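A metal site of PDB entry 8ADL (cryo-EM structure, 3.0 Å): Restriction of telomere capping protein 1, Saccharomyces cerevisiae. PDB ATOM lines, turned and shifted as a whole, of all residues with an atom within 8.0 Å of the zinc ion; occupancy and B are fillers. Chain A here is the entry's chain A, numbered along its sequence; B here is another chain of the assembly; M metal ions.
N of Leu 1295 sits close to SG of Cys 1293 (3.5 Å). N of Cys 1293 sits at hydrogen-bond distance from O of Arg 1298 (3.1 Å). N of Arg 1298 lies close to SG of Cys 1296, at 3.7 Å.
Four residues have an atom within 4 Å of the zinc ion: Cys 1293, Cys 1296, His 1315 and Cys 1318. The nearest printed residue that does not touch the zinc ion is Leu 1295 (4.9 Å).
The zinc ion is bound by a ring nitrogen (ND1) of His 1315 (2.1 Å), the side-chain sulfur (SG) of Cys 1318 (2.3 Å), the side-chain sulfur (SG) of Cys 1296 (2.3 Å) and the side-chain sulfur (SG) of Cys 1293 (2.3 Å). The zinc ion has four donor atoms within binding distance.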
ATOM      1  N   SER A1292      19.600  25.352 -15.627  1.00  0.00           N
ATOM      2  CA  SER A1292      20.751  25.896 -14.931  1.00  0.00           C
ATOM      3  C   SER A1292      22.006  25.078 -15.238  1.00  0.00           C
ATOM      4  O   SER A1292      21.940  23.867 -15.441  1.00  0.00           O
ATOM      5  CB  SER A1292      20.509  25.919 -13.425  1.00  0.00           C
ATOM      6  OG  SER A1292      19.440  26.790 -13.094  1.00  0.00           O
ATOM      7  N   CYS A1293      23.135  25.775 -15.297  1.00  0.00           N
ATOM      8  CA  CYS A1293      24.422  25.107 -15.483  1.00  0.00           C
ATOM      9  C   CYS A1293      24.762  24.265 -14.267  1.00  0.00           C
ATOM     10  O   CYS A1293      24.395  24.606 -13.132  1.00  0.00           O
ATOM     11  CB  CYS A1293      25.518  26.136 -15.747  1.00  0.00           C
ATOM     12  SG  CYS A1293      27.156  25.437 -16.075  1.00  0.00           S
ATOM     13  N   VAL A1294      25.453  23.160 -14.503  1.00  0.00           N
ATOM     14  CA  VAL A1294      25.789  22.245 -13.414  1.00  0.00           C
ATOM     15  C   VAL A1294      26.938  22.774 -12.553  1.00  0.00           C
ATOM     16  O   VAL A1294      27.117  22.324 -11.420  1.00  0.00           O
ATOM     17  CB  VAL A1294      26.102  20.859 -14.001  1.00  0.00           C
ATOM     18  CG1 VAL A1294      27.478  20.821 -14.646  1.00  0.00           C
ATOM     19  CG2 VAL A1294      25.935  19.758 -12.960  1.00  0.00           C
ATOM     20  N   LEU A1295      27.689  23.766 -13.043  1.00  0.00           N
ATOM     21  CA  LEU A1295      28.801  24.335 -12.302  1.00  0.00           C
ATOM     22  C   LEU A1295      28.498  25.723 -11.729  1.00  0.00           C
ATOM     23  O   LEU A1295      28.670  25.936 -10.528  1.00  0.00           O
ATOM     24  CB  LEU A1295      30.046  24.422 -13.197  1.00  0.00           C
ATOM     25  CG  LEU A1295      31.375  24.595 -12.460  1.00  0.00           C
ATOM     26  CD1 LEU A1295      31.681  23.396 -11.592  1.00  0.00           C
ATOM     27  CD2 LEU A1295      32.509  24.856 -13.432  1.00  0.00           C
ATOM     28  N   CYS A1296      28.041  26.656 -12.559  1.00  0.00           N
ATOM     29  CA  CYS A1296      27.845  28.040 -12.138  1.00  0.00           C
ATOM     30  C   CYS A1296      26.406  28.368 -11.775  1.00  0.00           C
ATOM     31  O   CYS A1296      26.165  29.460 -11.228  1.00  0.00           O
ATOM     32  CB  CYS A1296      28.326  28.996 -13.236  1.00  0.00           C
ATOM     33  SG  CYS A1296      27.372  28.943 -14.762  1.00  0.00           S
ATOM     34  N   GLU A1297      25.447  27.477 -12.065  1.00  0.00           N
ATOM     35  CA  GLU A1297      24.032  27.633 -11.722  1.00  0.00           C
ATOM     36  C   GLU A1297      23.414  28.895 -12.328  1.00  0.00           C
ATOM     37  O   GLU A1297      22.539  29.516 -11.726  1.00  0.00           O
ATOM     38  CB  GLU A1297      23.804  27.593 -10.211  1.00  0.00           C
ATOM     39  CG  GLU A1297      24.080  26.245  -9.571  1.00  0.00           C
ATOM     40  CD  GLU A1297      23.038  25.202  -9.926  1.00  0.00           C
ATOM     41  OE1 GLU A1297      21.851  25.573 -10.074  1.00  0.00           O
ATOM     42  OE2 GLU A1297      23.401  24.024 -10.050  1.00  0.00           O
ATOM     43  N   ARG A1298      23.884  29.285 -13.506  1.00  0.00           N
ATOM     44  CA  ARG A1298      23.394  30.410 -14.276  1.00  0.00           C
ATOM     45  C   ARG A1298      22.461  29.933 -15.375  1.00  0.00           C
ATOM     46  O   ARG A1298      22.459  28.743 -15.717  1.00  0.00           O
ATOM     47  CB  ARG A1298      24.576  31.184 -14.872  1.00  0.00           C
ATOM     48  CG  ARG A1298      25.179  32.224 -13.950  1.00  0.00           C
ATOM     49  CD  ARG A1298      26.410  32.853 -14.560  1.00  0.00           C
ATOM     50  NE  ARG A1298      27.426  33.180 -13.566  1.00  0.00           N
ATOM     51  CZ  ARG A1298      28.711  33.307 -13.819  1.00  0.00           C
ATOM     52  NH1 ARG A1298      29.197  33.132 -15.042  1.00  0.00           N
ATOM     53  NH2 ARG A1298      29.546  33.610 -12.828  1.00  0.00           N
ATOM     54  N   PRO A1299      21.617  30.802 -15.932  1.00  0.00           N
ATOM     55  CA  PRO A1299      20.746  30.385 -17.042  1.00  0.00           C
ATOM     56  C   PRO A1299      21.543  29.982 -18.275  1.00  0.00           C
ATOM     57  O   PRO A1299      22.630  30.499 -18.539  1.00  0.00           O
ATOM     58  CB  PRO A1299      19.884  31.633 -17.318  1.00  0.00           C
ATOM     59  CG  PRO A1299      20.570  32.748 -16.609  1.00  0.00           C
ATOM     60  CD  PRO A1299      21.210  32.130 -15.423  1.00  0.00           C
ATOM     61  N   LEU A1300      20.977  29.049 -19.034  1.00  0.00           N
ATOM     62  CA  LEU A1300      21.667  28.406 -20.140  1.00  0.00           C
ATOM     63  C   LEU A1300      20.725  28.354 -21.327  1.00  0.00           C
ATOM     64  O   LEU A1300      19.676  27.705 -21.259  1.00  0.00           O
ATOM     65  CB  LEU A1300      22.124  26.996 -19.739  1.00  0.00           C
ATOM     66  CG  LEU A1300      23.136  26.280 -20.625  1.00  0.00           C
ATOM     67  CD1 LEU A1300      24.250  27.218 -21.038  1.00  0.00           C
ATOM     68  CD2 LEU A1300      23.703  25.088 -19.876  1.00  0.00           C
ATOM     69  N   LEU A1303      24.114  27.395 -25.971  1.00  0.00           N
ATOM     70  CA  LEU A1303      24.985  26.252 -26.241  1.00  0.00           C
ATOM     71  C   LEU A1303      25.282  25.551 -24.926  1.00  0.00           C
ATOM     72  O   LEU A1303      25.671  26.197 -23.945  1.00  0.00           O
ATOM     73  CB  LEU A1303      26.298  26.676 -26.918  1.00  0.00           C
ATOM     74  CG  LEU A1303      26.402  26.560 -28.438  1.00  0.00           C
ATOM     75  CD1 LEU A1303      27.669  27.238 -28.942  1.00  0.00           C
ATOM     76  CD2 LEU A1303      26.360  25.110 -28.888  1.00  0.00           C
ATOM     77  N   GLU A1313      23.634  19.478 -18.046  1.00  0.00           N
ATOM     78  CA  GLU A1313      24.031  20.487 -19.020  1.00  0.00           C
ATOM     79  C   GLU A1313      25.324  21.161 -18.568  1.00  0.00           C
ATOM     80  O   GLU A1313      26.004  20.717 -17.634  1.00  0.00           O
ATOM     81  CB  GLU A1313      22.929  21.511 -19.227  1.00  0.00           C
ATOM     82  CG  GLU A1313      21.518  20.977 -19.317  1.00  0.00           C
ATOM     83  CD  GLU A1313      21.099  20.623 -20.716  1.00  0.00           C
ATOM     84  OE1 GLU A1313      21.876  20.860 -21.658  1.00  0.00           O
ATOM     85  OE2 GLU A1313      19.959  20.154 -20.891  1.00  0.00           O
ATOM     86  N   GLY A1314      25.674  22.260 -19.225  1.00  0.00           N
ATOM     87  CA  GLY A1314      26.818  23.074 -18.830  1.00  0.00           C
ATOM     88  C   GLY A1314      27.368  23.884 -19.977  1.00  0.00           C
ATOM     89  O   GLY A1314      27.288  23.461 -21.129  1.00  0.00           O
ATOM     90  N   HIS A1315      27.947  25.047 -19.682  1.00  0.00           N
ATOM     91  CA  HIS A1315      28.605  25.847 -20.703  1.00  0.00           C
ATOM     92  C   HIS A1315      29.866  25.147 -21.205  1.00  0.00           C
ATOM     93  O   HIS A1315      30.359  24.192 -20.592  1.00  0.00           O
ATOM     94  CB  HIS A1315      28.979  27.225 -20.164  1.00  0.00           C
ATOM     95  CG  HIS A1315      27.821  28.010 -19.626  1.00  0.00           C
ATOM     96  ND1 HIS A1315      27.282  27.784 -18.382  1.00  0.00           N
ATOM     97  CD2 HIS A1315      27.130  29.045 -20.150  1.00  0.00           C
ATOM     98  CE1 HIS A1315      26.290  28.631 -18.169  1.00  0.00           C
ATOM     99  NE2 HIS A1315      26.170  29.410 -19.230  1.00  0.00           N
ATOM    100  N   PHE A1316      30.375  25.628 -22.344  1.00  0.00           N
ATOM    101  CA  PHE A1316      31.690  25.182 -22.793  1.00  0.00           C
ATOM    102  C   PHE A1316      32.772  25.550 -21.795  1.00  0.00           C
ATOM    103  O   PHE A1316      33.616  24.720 -21.432  1.00  0.00           O
ATOM    104  CB  PHE A1316      32.019  25.756 -24.172  1.00  0.00           C
ATOM    105  CG  PHE A1316      31.202  25.202 -25.298  1.00  0.00           C
ATOM    106  CD1 PHE A1316      30.463  24.034 -25.146  1.00  0.00           C
ATOM    107  CD2 PHE A1316      31.181  25.832 -26.532  1.00  0.00           C
ATOM    108  CE1 PHE A1316      29.731  23.522 -26.188  1.00  0.00           C
ATOM    109  CE2 PHE A1316      30.438  25.321 -27.583  1.00  0.00           C
ATOM    110  CZ  PHE A1316      29.710  24.170 -27.405  1.00  0.00           C
ATOM    111  N   GLN A1317      32.749  26.796 -21.314  1.00  0.00           N
ATOM    112  CA  GLN A1317      33.797  27.277 -20.426  1.00  0.00           C
ATOM    113  C   GLN A1317      33.757  26.568 -19.079  1.00  0.00           C
ATOM    114  O   GLN A1317      34.805  26.179 -18.550  1.00  0.00           O
ATOM    115  CB  GLN A1317      33.688  28.793 -20.246  1.00  0.00           C
ATOM    116  CG  GLN A1317      34.914  29.435 -19.629  1.00  0.00           C
ATOM    117  CD  GLN A1317      36.134  29.336 -20.519  1.00  0.00           C
ATOM    118  OE1 GLN A1317      36.049  29.475 -21.735  1.00  0.00           O
ATOM    119  NE2 GLN A1317      37.297  29.091 -19.909  1.00  0.00           N
ATOM    120  N   CYS A1318      32.561  26.358 -18.524  1.00  0.00           N
ATOM    121  CA  CYS A1318      32.422  25.729 -17.209  1.00  0.00           C
ATOM    122  C   CYS A1318      32.867  24.269 -17.240  1.00  0.00           C
ATOM    123  O   CYS A1318      33.675  23.832 -16.404  1.00  0.00           O
ATOM    124  CB  CYS A1318      30.974  25.836 -16.737  1.00  0.00           C
ATOM    125  SG  CYS A1318      30.379  27.524 -16.542  1.00  0.00           S
ATOM    126  N   ILE A1319      32.350  23.500 -18.208  1.00  0.00           N
ATOM    127  CA  ILE A1319      32.686  22.088 -18.333  1.00  0.00           C
ATOM    128  C   ILE A1319      34.169  21.911 -18.677  1.00  0.00           C
ATOM    129  O   ILE A1319      34.846  21.046 -18.124  1.00  0.00           O
ATOM    130  CB  ILE A1319      31.764  21.420 -19.370  1.00  0.00           C
ATOM    131  CG1 ILE A1319      30.327  21.363 -18.853  1.00  0.00           C
ATOM    132  CG2 ILE A1319      32.242  20.025 -19.727  1.00  0.00           C
ATOM    133  CD1 ILE A1319      30.173  20.557 -17.590  1.00  0.00           C
ATOM    134  N   GLU A1321      36.639  24.035 -17.987  1.00  0.00           N
ATOM    135  CA  GLU A1321      37.425  24.380 -16.803  1.00  0.00           C
ATOM    136  C   GLU A1321      37.414  23.239 -15.800  1.00  0.00           C
ATOM    137  O   GLU A1321      38.469  22.843 -15.281  1.00  0.00           O
ATOM    138  CB  GLU A1321      36.873  25.661 -16.171  1.00  0.00           C
ATOM    139  CG  GLU A1321      37.462  26.947 -16.727  1.00  0.00           C
ATOM    140  CD  GLU A1321      36.788  28.177 -16.157  1.00  0.00           C
ATOM    141  OE1 GLU A1321      35.757  28.023 -15.476  1.00  0.00           O
ATOM    142  OE2 GLU A1321      37.294  29.297 -16.377  1.00  0.00           O
ATOM    143  N   PHE B 847      32.764  28.155  -7.666  1.00  0.00           N
ATOM    144  CA  PHE B 847      31.911  27.100  -8.213  1.00  0.00           C
ATOM    145  C   PHE B 847      32.622  25.745  -8.232  1.00  0.00           C
ATOM    146  O   PHE B 847      31.988  24.710  -8.037  1.00  0.00           O
ATOM    147  CB  PHE B 847      31.450  27.491  -9.612  1.00  0.00           C
ATOM    148  CG  PHE B 847      30.763  28.819  -9.665  1.00  0.00           C
ATOM    149  CD1 PHE B 847      29.602  29.051  -8.957  1.00  0.00           C
ATOM    150  CD2 PHE B 847      31.281  29.851 -10.441  1.00  0.00           C
ATOM    151  CE1 PHE B 847      28.965  30.276  -9.004  1.00  0.00           C
ATOM    152  CE2 PHE B 847      30.657  31.080 -10.492  1.00  0.00           C
ATOM    153  CZ  PHE B 847      29.500  31.293  -9.768  1.00  0.00           C
HETATM  154 ZN    ZN M   1      28.067  27.533 -16.461  1.00  0.00          ZN
